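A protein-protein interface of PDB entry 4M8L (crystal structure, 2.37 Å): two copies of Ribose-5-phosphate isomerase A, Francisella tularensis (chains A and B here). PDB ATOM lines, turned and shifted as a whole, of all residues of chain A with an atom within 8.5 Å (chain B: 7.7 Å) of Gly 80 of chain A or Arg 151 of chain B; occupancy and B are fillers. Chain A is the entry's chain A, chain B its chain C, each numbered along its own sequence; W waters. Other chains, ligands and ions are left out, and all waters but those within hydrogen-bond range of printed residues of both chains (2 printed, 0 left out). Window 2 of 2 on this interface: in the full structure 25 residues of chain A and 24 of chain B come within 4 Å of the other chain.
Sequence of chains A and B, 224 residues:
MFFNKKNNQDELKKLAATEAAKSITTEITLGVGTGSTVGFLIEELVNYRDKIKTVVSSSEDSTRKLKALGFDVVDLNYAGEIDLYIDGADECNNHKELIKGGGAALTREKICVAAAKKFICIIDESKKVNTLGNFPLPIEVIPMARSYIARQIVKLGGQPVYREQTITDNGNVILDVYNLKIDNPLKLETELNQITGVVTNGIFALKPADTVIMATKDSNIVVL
Among the printed residues, merely in contact across the chains: Leu 76 of chain A with Met 144 of chain B (3.6 Å), Asn 77 of chain A with Met 144 of chain B (3.8 Å), Asn 77 of chain A with Arg 146 of chain B (3.6 Å), Gly 80 of chain A with Arg 151 of chain B (3.7 Å), Ile 111 of chain A with Ala 145 of chain B (3.7 Å), Cys 112 of chain A with Met 144 of chain B (3.4 Å) and Ala 114 of chain A with Tyr 148 of chain B (3.8 Å).
Of the 17 printed residues of chain B, 6 touch a printed residue of chain A.
Hydrophobic or aromatic side chains of chain B within 4 Å of the printed part of chain A: Met 144, Ala 145 and Tyr 148.
Along chain B the printed residues that touch a printed residue of chain A span positions 144 to 151.
Of the 18 printed residues of chain A, 6 touch a printed residue of chain B.
Among the printed residues, 8 pairs touch across the chains.
Among the printed residues, no Asp or Glu carboxylate lies within 4 Å of a Lys or Arg side-chain nitrogen of the other chain.
No position is printed for both chains.
The side-chain hydroxyl of Ser 147 of chain B sits at hydrogen-bond distance from the side-chain amide oxygen of Asn 77 of chain A (2.7 Å).
NE2 of Gln 152 of chain B sits close to O of Tyr 148 of chain B (3.5 Å).
The side-chain amide nitrogen (ND2) of Asn 77 of chain A sits at hydrogen-bond distance from the side-chain carboxylate (OD2) of Asp 75 of chain A, 3.0 Å away.
O of Ser 147 of chain B lies within hydrogen-bond range of NH1 of Arg 151 of chain B (3.4 Å).
Of the printed residues of chain B, Asn 77 of chain A touches Met 144 (3.8 Å), Arg 146 (3.6 Å) and Ser 147 (2.7 Å).
No residue of chain B comes within 4 Å of Ala 79 of chain A.
Printed residues of chain B within 4 Å of Gly 80 of chain A: Arg 151 (3.7 Å).
Of the printed residues of chain B, Ile 111 of chain A touches Ala 145 (3.7 Å).
Of the printed residues of chain B, Cys 112 of chain A touches Met 144 (3.4 Å).
Printed residues of chain B within 4 Å of Ala 114 of chain A: Tyr 148 (3.8 Å).
Ala 115 of chain A touches none of the printed residues of chain B.
Printed residues of chain A within 4 Å of Tyr 148 of chain B: Ala 114 (3.8 Å).
No residue of chain A comes within 4 Å of Ala 150 of chain B.
Of chain A, only Gly 80 (3.7 Å) comes within 4 Å of Arg 151 of chain B.
The nearest residue of chain A that does not touch Arg 151 of chain B is Glu 81 of chain A (4.9 Å).
The nearest printed residue of chain A that does not touch Met 144 of chain B is Val 56 of chain A (4.1 Å).
Water W1 lies within hydrogen-bond range of O of Met 144 of chain B (2.8 Å), N of Tyr 148 of chain B (3.0 Å), N of Ser 147 of chain B (3.2 Å) and OD1 of Asn 77 of chain A (3.2 Å).
Water W2 lies within hydrogen-bond range of the backbone carbonyl oxygen of Gly 80 of chain A (2.9 Å), the backbone carbonyl oxygen of Leu 76 of chain A (3.1 Å) and the guanidinium group of Arg 151 of chain B (3.2 Å).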
ATOM      1  N   THR A  29     -26.159  -2.286 -21.824  1.00  0.00           N
ATOM      2  CA  THR A  29     -25.503  -2.754 -23.037  1.00  0.00           C
ATOM      3  C   THR A  29     -25.043  -4.176 -22.741  1.00  0.00           C
ATOM      4  O   THR A  29     -24.187  -4.382 -21.878  1.00  0.00           O
ATOM      5  CB  THR A  29     -24.298  -1.866 -23.415  1.00  0.00           C
ATOM      6  OG1 THR A  29     -24.762  -0.563 -23.787  1.00  0.00           O
ATOM      7  CG2 THR A  29     -23.509  -2.460 -24.581  1.00  0.00           C
ATOM      8  N   THR A  54     -28.842  -2.194 -25.895  1.00  0.00           N
ATOM      9  CA  THR A  54     -27.890  -2.406 -26.979  1.00  0.00           C
ATOM     10  C   THR A  54     -27.227  -3.781 -26.853  1.00  0.00           C
ATOM     11  O   THR A  54     -26.880  -4.206 -25.750  1.00  0.00           O
ATOM     12  CB  THR A  54     -26.787  -1.327 -26.961  1.00  0.00           C
ATOM     13  OG1 THR A  54     -27.350  -0.058 -26.604  1.00  0.00           O
ATOM     14  CG2 THR A  54     -26.115  -1.216 -28.315  1.00  0.00           C
ATOM     15  N   VAL A  56     -24.010  -6.234 -28.251  1.00  0.00           N
ATOM     16  CA  VAL A  56     -22.725  -6.363 -28.945  1.00  0.00           C
ATOM     17  C   VAL A  56     -22.405  -7.858 -29.025  1.00  0.00           C
ATOM     18  O   VAL A  56     -22.650  -8.608 -28.078  1.00  0.00           O
ATOM     19  CB  VAL A  56     -21.571  -5.619 -28.213  1.00  0.00           C
ATOM     20  CG1 VAL A  56     -20.345  -5.547 -29.108  1.00  0.00           C
ATOM     21  CG2 VAL A  56     -21.958  -4.203 -27.780  1.00  0.00           C
ATOM     22  N   VAL A  74     -25.099  -4.004 -32.535  1.00  0.00           N
ATOM     23  CA  VAL A  74     -24.343  -2.767 -32.712  1.00  0.00           C
ATOM     24  C   VAL A  74     -22.850  -3.045 -32.576  1.00  0.00           C
ATOM     25  O   VAL A  74     -22.427  -3.810 -31.710  1.00  0.00           O
ATOM     26  CB  VAL A  74     -24.770  -1.699 -31.679  1.00  0.00           C
ATOM     27  CG1 VAL A  74     -23.987  -0.407 -31.878  1.00  0.00           C
ATOM     28  CG2 VAL A  74     -26.266  -1.427 -31.780  1.00  0.00           C
ATOM     29  N   ASP A  75     -22.064  -2.428 -33.455  1.00  0.00           N
ATOM     30  CA  ASP A  75     -20.606  -2.538 -33.436  1.00  0.00           C
ATOM     31  C   ASP A  75     -20.050  -1.988 -32.121  1.00  0.00           C
ATOM     32  O   ASP A  75     -20.587  -1.022 -31.575  1.00  0.00           O
ATOM     33  CB  ASP A  75     -20.016  -1.759 -34.618  1.00  0.00           C
ATOM     34  CG  ASP A  75     -18.548  -2.027 -34.819  1.00  0.00           C
ATOM     35  OD1 ASP A  75     -18.208  -3.088 -35.382  1.00  0.00           O
ATOM     36  OD2 ASP A  75     -17.730  -1.177 -34.416  1.00  0.00           O
ATOM     37  N   LEU A  76     -18.974  -2.592 -31.623  1.00  0.00           N
ATOM     38  CA  LEU A  76     -18.382  -2.191 -30.339  1.00  0.00           C
ATOM     39  C   LEU A  76     -17.892  -0.733 -30.325  1.00  0.00           C
ATOM     40  O   LEU A  76     -17.908  -0.091 -29.276  1.00  0.00           O
ATOM     41  CB  LEU A  76     -17.234  -3.134 -29.952  1.00  0.00           C
ATOM     42  CG  LEU A  76     -16.552  -2.902 -28.595  1.00  0.00           C
ATOM     43  CD1 LEU A  76     -17.550  -2.918 -27.448  1.00  0.00           C
ATOM     44  CD2 LEU A  76     -15.469  -3.946 -28.359  1.00  0.00           C
ATOM     45  N   ASN A  77     -17.462  -0.228 -31.481  1.00  0.00           N
ATOM     46  CA  ASN A  77     -17.007   1.162 -31.604  1.00  0.00           C
ATOM     47  C   ASN A  77     -18.116   2.198 -31.385  1.00  0.00           C
ATOM     48  O   ASN A  77     -17.837   3.303 -30.916  1.00  0.00           O
ATOM     49  CB  ASN A  77     -16.355   1.407 -32.969  1.00  0.00           C
ATOM     50  CG  ASN A  77     -15.008   0.724 -33.105  1.00  0.00           C
ATOM     51  OD1 ASN A  77     -14.076   1.031 -32.363  1.00  0.00           O
ATOM     52  ND2 ASN A  77     -14.897  -0.208 -34.052  1.00  0.00           N
ATOM     53  N   TYR A  78     -19.355   1.847 -31.732  1.00  0.00           N
ATOM     54  CA  TYR A  78     -20.509   2.729 -31.522  1.00  0.00           C
ATOM     55  C   TYR A  78     -21.204   2.447 -30.194  1.00  0.00           C
ATOM     56  O   TYR A  78     -21.904   3.307 -29.674  1.00  0.00           O
ATOM     57  CB  TYR A  78     -21.538   2.556 -32.637  1.00  0.00           C
ATOM     58  CG  TYR A  78     -22.463   3.740 -32.842  1.00  0.00           C
ATOM     59  CD1 TYR A  78     -22.166   4.731 -33.778  1.00  0.00           C
ATOM     60  CD2 TYR A  78     -23.649   3.862 -32.112  1.00  0.00           C
ATOM     61  CE1 TYR A  78     -23.014   5.812 -33.971  1.00  0.00           C
ATOM     62  CE2 TYR A  78     -24.501   4.940 -32.299  1.00  0.00           C
ATOM     63  CZ  TYR A  78     -24.180   5.912 -33.228  1.00  0.00           C
ATOM     64  OH  TYR A  78     -25.026   6.981 -33.416  1.00  0.00           O
ATOM     65  N   ALA A  79     -21.039   1.236 -29.670  1.00  0.00           N
ATOM     66  CA  ALA A  79     -21.634   0.861 -28.389  1.00  0.00           C
ATOM     67  C   ALA A  79     -20.847   1.461 -27.228  1.00  0.00           C
ATOM     68  O   ALA A  79     -21.423   1.873 -26.218  1.00  0.00           O
ATOM     69  CB  ALA A  79     -21.686  -0.652 -28.258  1.00  0.00           C
ATOM     70  N   GLY A  80     -19.524   1.491 -27.377  1.00  0.00           N
ATOM     71  CA  GLY A  80     -18.633   2.022 -26.355  1.00  0.00           C
ATOM     72  C   GLY A  80     -18.224   0.959 -25.357  1.00  0.00           C
ATOM     73  O   GLY A  80     -17.362   0.122 -25.638  1.00  0.00           O
ATOM     74  N   GLU A  81     -18.848   0.991 -24.186  1.00  0.00           N
ATOM     75  CA  GLU A  81     -18.482   0.112 -23.090  1.00  0.00           C
ATOM     76  C   GLU A  81     -19.617  -0.860 -22.812  1.00  0.00           C
ATOM     77  O   GLU A  81     -20.776  -0.459 -22.762  1.00  0.00           O
ATOM     78  CB  GLU A  81     -18.190   0.971 -21.857  1.00  0.00           C
ATOM     79  CG  GLU A  81     -17.904   0.223 -20.567  1.00  0.00           C
ATOM     80  CD  GLU A  81     -17.589   1.158 -19.409  1.00  0.00           C
ATOM     81  OE1 GLU A  81     -18.506   1.807 -18.855  1.00  0.00           O
ATOM     82  OE2 GLU A  81     -16.399   1.246 -19.054  1.00  0.00           O
ATOM     83  N   ILE A  82     -19.281  -2.132 -22.618  1.00  0.00           N
ATOM     84  CA  ILE A  82     -20.277  -3.154 -22.315  1.00  0.00           C
ATOM     85  C   ILE A  82     -20.468  -3.228 -20.800  1.00  0.00           C
ATOM     86  O   ILE A  82     -19.491  -3.255 -20.052  1.00  0.00           O
ATOM     87  CB  ILE A  82     -19.851  -4.541 -22.847  1.00  0.00           C
ATOM     88  CG1 ILE A  82     -19.540  -4.473 -24.347  1.00  0.00           C
ATOM     89  CG2 ILE A  82     -20.943  -5.570 -22.588  1.00  0.00           C
ATOM     90  CD1 ILE A  82     -18.718  -5.644 -24.849  1.00  0.00           C
ATOM     91  N   ASP A  83     -21.721  -3.262 -20.352  1.00  0.00           N
ATOM     92  CA  ASP A  83     -22.025  -3.375 -18.921  1.00  0.00           C
ATOM     93  C   ASP A  83     -21.864  -4.817 -18.455  1.00  0.00           C
ATOM     94  O   ASP A  83     -21.270  -5.078 -17.406  1.00  0.00           O
ATOM     95  CB  ASP A  83     -23.449  -2.898 -18.620  1.00  0.00           C
ATOM     96  CG  ASP A  83     -23.674  -1.438 -18.988  1.00  0.00           C
ATOM     97  OD1 ASP A  83     -22.784  -0.599 -18.722  1.00  0.00           O
ATOM     98  OD2 ASP A  83     -24.750  -1.129 -19.541  1.00  0.00           O
ATOM     99  N   ILE A 111     -11.607  -9.197 -26.664  1.00  0.00           N
ATOM    100  CA  ILE A 111     -11.868  -7.768 -26.792  1.00  0.00           C
ATOM    101  C   ILE A 111     -13.137  -7.388 -26.017  1.00  0.00           C
ATOM    102  O   ILE A 111     -13.149  -6.396 -25.286  1.00  0.00           O
ATOM    103  CB  ILE A 111     -11.995  -7.346 -28.278  1.00  0.00           C
ATOM    104  CG1 ILE A 111     -10.650  -7.515 -29.000  1.00  0.00           C
ATOM    105  CG2 ILE A 111     -12.456  -5.897 -28.394  1.00  0.00           C
ATOM    106  CD1 ILE A 111     -10.756  -7.616 -30.512  1.00  0.00           C
ATOM    107  N   CYS A 112     -14.194  -8.181 -26.171  1.00  0.00           N
ATOM    108  CA  CYS A 112     -15.443  -7.941 -25.441  1.00  0.00           C
ATOM    109  C   CYS A 112     -15.250  -8.008 -23.929  1.00  0.00           C
ATOM    110  O   CYS A 112     -15.801  -7.181 -23.197  1.00  0.00           O
ATOM    111  CB  CYS A 112     -16.523  -8.931 -25.865  1.00  0.00           C
ATOM    112  SG  CYS A 112     -17.230  -8.588 -27.483  1.00  0.00           S
ATOM    113  N   ALA A 114     -12.461  -7.432 -22.359  1.00  0.00           N
ATOM    114  CA  ALA A 114     -11.633  -6.281 -22.002  1.00  0.00           C
ATOM    115  C   ALA A 114     -12.455  -5.003 -21.862  1.00  0.00           C
ATOM    116  O   ALA A 114     -12.180  -4.180 -20.995  1.00  0.00           O
ATOM    117  CB  ALA A 114     -10.525  -6.090 -23.029  1.00  0.00           C
ATOM    118  N   ALA A 115     -13.462  -4.849 -22.715  1.00  0.00           N
ATOM    119  CA  ALA A 115     -14.326  -3.664 -22.709  1.00  0.00           C
ATOM    120  C   ALA A 115     -15.573  -3.816 -21.826  1.00  0.00           C
ATOM    121  O   ALA A 115     -16.427  -2.930 -21.816  1.00  0.00           O
ATOM    122  CB  ALA A 115     -14.740  -3.324 -24.133  1.00  0.00           C
ATOM    123  N   ALA A 116     -15.676  -4.919 -21.081  1.00  0.00           N
ATOM    124  CA  ALA A 116     -16.855  -5.181 -20.251  1.00  0.00           C
ATOM    125  C   ALA A 116     -16.600  -4.830 -18.789  1.00  0.00           C
ATOM    126  O   ALA A 116     -15.551  -5.166 -18.236  1.00  0.00           O
ATOM    127  CB  ALA A 116     -17.277  -6.642 -20.371  1.00  0.00           C
ATOM    128  N   MET B 144     -12.727  -3.949 -34.588  1.00  0.00           N
ATOM    129  CA  MET B 144     -13.669  -3.934 -33.467  1.00  0.00           C
ATOM    130  C   MET B 144     -13.118  -3.285 -32.189  1.00  0.00           C
ATOM    131  O   MET B 144     -13.883  -2.738 -31.401  1.00  0.00           O
ATOM    132  CB  MET B 144     -14.111  -5.370 -33.156  1.00  0.00           C
ATOM    133  CG  MET B 144     -15.055  -5.508 -31.974  1.00  0.00           C
ATOM    134  SD  MET B 144     -15.483  -7.224 -31.650  1.00  0.00           S
ATOM    135  CE  MET B 144     -16.736  -6.984 -30.397  1.00  0.00           C
ATOM    136  N   ALA B 145     -11.806  -3.353 -31.986  1.00  0.00           N
ATOM    137  CA  ALA B 145     -11.179  -2.869 -30.750  1.00  0.00           C
ATOM    138  C   ALA B 145     -10.634  -1.443 -30.851  1.00  0.00           C
ATOM    139  O   ALA B 145      -9.987  -0.963 -29.920  1.00  0.00           O
ATOM    140  CB  ALA B 145     -10.058  -3.816 -30.345  1.00  0.00           C
ATOM    141  N   ARG B 146     -10.875  -0.769 -31.974  1.00  0.00           N
ATOM    142  CA  ARG B 146     -10.229   0.521 -32.239  1.00  0.00           C
ATOM    143  C   ARG B 146     -10.510   1.563 -31.151  1.00  0.00           C
ATOM    144  O   ARG B 146      -9.589   2.203 -30.640  1.00  0.00           O
ATOM    145  CB  ARG B 146     -10.653   1.062 -33.605  1.00  0.00           C
ATOM    146  CG  ARG B 146      -9.938   2.340 -34.009  1.00  0.00           C
ATOM    147  CD  ARG B 146     -10.211   2.679 -35.458  1.00  0.00           C
ATOM    148  NE  ARG B 146     -11.641   2.916 -35.670  1.00  0.00           N
ATOM    149  CZ  ARG B 146     -12.277   4.048 -35.375  1.00  0.00           C
ATOM    150  NH1 ARG B 146     -11.624   5.085 -34.859  1.00  0.00           N
ATOM    151  NH2 ARG B 146     -13.576   4.149 -35.610  1.00  0.00           N
ATOM    152  N   SER B 147     -11.783   1.722 -30.802  1.00  0.00           N
ATOM    153  CA  SER B 147     -12.179   2.707 -29.797  1.00  0.00           C
ATOM    154  C   SER B 147     -11.640   2.351 -28.409  1.00  0.00           C
ATOM    155  O   SER B 147     -11.165   3.226 -27.686  1.00  0.00           O
ATOM    156  CB  SER B 147     -13.699   2.857 -29.762  1.00  0.00           C
ATOM    157  OG  SER B 147     -14.167   3.374 -30.999  1.00  0.00           O
ATOM    158  N   TYR B 148     -11.709   1.072 -28.046  1.00  0.00           N
ATOM    159  CA  TYR B 148     -11.166   0.606 -26.770  1.00  0.00           C
ATOM    160  C   TYR B 148      -9.667   0.884 -26.666  1.00  0.00           C
ATOM    161  O   TYR B 148      -9.194   1.401 -25.653  1.00  0.00           O
ATOM    162  CB  TYR B 148     -11.428  -0.891 -26.570  1.00  0.00           C
ATOM    163  CG  TYR B 148     -10.634  -1.471 -25.426  1.00  0.00           C
ATOM    164  CD1 TYR B 148     -10.974  -1.191 -24.107  1.00  0.00           C
ATOM    165  CD2 TYR B 148      -9.525  -2.287 -25.663  1.00  0.00           C
ATOM    166  CE1 TYR B 148     -10.239  -1.712 -23.055  1.00  0.00           C
ATOM    167  CE2 TYR B 148      -8.787  -2.809 -24.618  1.00  0.00           C
ATOM    168  CZ  TYR B 148      -9.147  -2.517 -23.317  1.00  0.00           C
ATOM    169  OH  TYR B 148      -8.410  -3.030 -22.278  1.00  0.00           O
ATOM    170  N   ILE B 149      -8.932   0.547 -27.722  1.00  0.00           N
ATOM    171  CA  ILE B 149      -7.477   0.722 -27.742  1.00  0.00           C
ATOM    172  C   ILE B 149      -7.095   2.195 -27.749  1.00  0.00           C
ATOM    173  O   ILE B 149      -6.144   2.595 -27.073  1.00  0.00           O
ATOM    174  CB  ILE B 149      -6.840   0.002 -28.947  1.00  0.00           C
ATOM    175  CG1 ILE B 149      -6.971  -1.511 -28.772  1.00  0.00           C
ATOM    176  CG2 ILE B 149      -5.368   0.380 -29.101  1.00  0.00           C
ATOM    177  CD1 ILE B 149      -6.747  -2.295 -30.047  1.00  0.00           C
ATOM    178  N   ALA B 150      -7.832   2.997 -28.514  1.00  0.00           N
ATOM    179  CA  ALA B 150      -7.633   4.449 -28.519  1.00  0.00           C
ATOM    180  C   ALA B 150      -7.676   5.005 -27.093  1.00  0.00           C
ATOM    181  O   ALA B 150      -6.819   5.801 -26.712  1.00  0.00           O
ATOM    182  CB  ALA B 150      -8.685   5.128 -29.384  1.00  0.00           C
ATOM    183  N   ARG B 151      -8.663   4.567 -26.310  1.00  0.00           N
ATOM    184  CA  ARG B 151      -8.788   4.984 -24.910  1.00  0.00           C
ATOM    185  C   ARG B 151      -7.593   4.544 -24.060  1.00  0.00           C
ATOM    186  O   ARG B 151      -7.088   5.327 -23.255  1.00  0.00           O
ATOM    187  CB  ARG B 151     -10.092   4.459 -24.286  1.00  0.00           C
ATOM    188  CG  ARG B 151     -11.337   5.213 -24.738  1.00  0.00           C
ATOM    189  CD  ARG B 151     -12.523   4.961 -23.826  1.00  0.00           C
ATOM    190  NE  ARG B 151     -13.015   3.587 -23.915  1.00  0.00           N
ATOM    191  CZ  ARG B 151     -13.738   3.091 -24.921  1.00  0.00           C
ATOM    192  NH1 ARG B 151     -14.081   3.847 -25.959  1.00  0.00           N
ATOM    193  NH2 ARG B 151     -14.118   1.815 -24.891  1.00  0.00           N
ATOM    194  N   GLN B 152      -7.135   3.304 -24.241  1.00  0.00           N
ATOM    195  CA  GLN B 152      -5.969   2.819 -23.491  1.00  0.00           C
ATOM    196  C   GLN B 152      -4.700   3.596 -23.839  1.00  0.00           C
ATOM    197  O   GLN B 152      -3.841   3.794 -22.983  1.00  0.00           O
ATOM    198  CB  GLN B 152      -5.718   1.324 -23.717  1.00  0.00           C
ATOM    199  CG  GLN B 152      -6.872   0.399 -23.356  1.00  0.00           C
ATOM    200  CD  GLN B 152      -7.583   0.793 -22.066  1.00  0.00           C
ATOM    201  OE1 GLN B 152      -6.998   0.769 -20.981  1.00  0.00           O
ATOM    202  NE2 GLN B 152      -8.858   1.144 -22.181  1.00  0.00           N
ATOM    203  N   ILE B 153      -4.593   4.033 -25.091  1.00  0.00           N
ATOM    204  CA  ILE B 153      -3.462   4.842 -25.534  1.00  0.00           C
ATOM    205  C   ILE B 153      -3.532   6.264 -24.957  1.00  0.00           C
ATOM    206  O   ILE B 153      -2.500   6.852 -24.625  1.00  0.00           O
ATOM    207  CB  ILE B 153      -3.355   4.861 -27.078  1.00  0.00           C
ATOM    208  CG1 ILE B 153      -2.920   3.481 -27.569  1.00  0.00           C
ATOM    209  CG2 ILE B 153      -2.357   5.915 -27.549  1.00  0.00           C
ATOM    210  CD1 ILE B 153      -3.102   3.256 -29.053  1.00  0.00           C
ATOM    211  N   VAL B 154      -4.740   6.811 -24.835  1.00  0.00           N
ATOM    212  CA  VAL B 154      -4.922   8.108 -24.173  1.00  0.00           C
ATOM    213  C   VAL B 154      -4.448   8.054 -22.705  1.00  0.00           C
ATOM    214  O   VAL B 154      -3.835   9.005 -22.225  1.00  0.00           O
ATOM    215  CB  VAL B 154      -6.386   8.607 -24.277  1.00  0.00           C
ATOM    216  CG1 VAL B 154      -6.633   9.811 -23.373  1.00  0.00           C
ATOM    217  CG2 VAL B 154      -6.729   8.957 -25.722  1.00  0.00           C
ATOM    218  N   LYS B 155      -4.716   6.946 -22.007  1.00  0.00           N
ATOM    219  CA  LYS B 155      -4.252   6.769 -20.619  1.00  0.00           C
ATOM    220  C   LYS B 155      -2.730   6.846 -20.493  1.00  0.00           C
ATOM    221  O   LYS B 155      -2.207   7.373 -19.516  1.00  0.00           O
ATOM    222  CB  LYS B 155      -4.720   5.427 -20.042  1.00  0.00           C
ATOM    223  CG  LYS B 155      -6.206   5.329 -19.747  1.00  0.00           C
ATOM    224  CD  LYS B 155      -6.507   4.106 -18.890  1.00  0.00           C
ATOM    225  CE  LYS B 155      -8.001   3.839 -18.793  1.00  0.00           C
ATOM    226  NZ  LYS B 155      -8.335   2.711 -17.879  1.00  0.00           N
ATOM    227  N   LEU B 156      -2.026   6.315 -21.489  1.00  0.00           N
ATOM    228  CA  LEU B 156      -0.561   6.328 -21.512  1.00  0.00           C
ATOM    229  C   LEU B 156       0.025   7.688 -21.888  1.00  0.00           C
ATOM    230  O   LEU B 156       1.239   7.875 -21.812  1.00  0.00           O
ATOM    231  CB  LEU B 156      -0.038   5.278 -22.499  1.00  0.00           C
ATOM    232  CG  LEU B 156      -0.471   3.829 -22.277  1.00  0.00           C
ATOM    233  CD1 LEU B 156      -0.127   2.984 -23.493  1.00  0.00           C
ATOM    234  CD2 LEU B 156       0.175   3.264 -21.024  1.00  0.00           C
ATOM    235  N   GLY B 157      -0.824   8.629 -22.301  1.00  0.00           N
ATOM    236  CA  GLY B 157      -0.373   9.967 -22.699  1.00  0.00           C
ATOM    237  C   GLY B 157      -0.240  10.152 -24.203  1.00  0.00           C
ATOM    238  O   GLY B 157       0.084  11.246 -24.672  1.00  0.00           O
ATOM    239  N   GLY B 158      -0.496   9.090 -24.964  1.00  0.00           N
ATOM    240  CA  GLY B 158      -0.448   9.162 -26.417  1.00  0.00           C
ATOM    241  C   GLY B 158      -1.708   9.778 -26.995  1.00  0.00           C
ATOM    242  O   GLY B 158      -2.743   9.834 -26.334  1.00  0.00           O
ATOM    243  N   PRO B 160      -3.944   9.055 -30.244  1.00  0.00           N
ATOM    244  CA  PRO B 160      -4.121   8.175 -31.397  1.00  0.00           C
ATOM    245  C   PRO B 160      -4.963   8.801 -32.503  1.00  0.00           C
ATOM    246  O   PRO B 160      -6.020   9.357 -32.226  1.00  0.00           O
ATOM    247  CB  PRO B 160      -4.847   6.967 -30.799  1.00  0.00           C
ATOM    248  CG  PRO B 160      -5.654   7.548 -29.690  1.00  0.00           C
ATOM    249  CD  PRO B 160      -4.887   8.730 -29.158  1.00  0.00           C
ATOM    250  N   LEU B 175      -3.753   2.758 -36.113  1.00  0.00           N
ATOM    251  CA  LEU B 175      -3.747   3.965 -35.291  1.00  0.00           C
ATOM    252  C   LEU B 175      -2.328   4.535 -35.285  1.00  0.00           C
ATOM    253  O   LEU B 175      -1.378   3.827 -34.940  1.00  0.00           O
ATOM    254  CB  LEU B 175      -4.160   3.645 -33.853  1.00  0.00           C
ATOM    255  CG  LEU B 175      -5.617   3.266 -33.590  1.00  0.00           C
ATOM    256  CD1 LEU B 175      -5.763   2.726 -32.180  1.00  0.00           C
ATOM    257  CD2 LEU B 175      -6.549   4.450 -33.801  1.00  0.00           C
HETATM  258  O   HOH W   1     -13.594  -0.614 -29.675  1.00  0.00           O
HETATM  259  O   HOH W   2     -15.336   0.603 -27.628  1.00  0.00           O
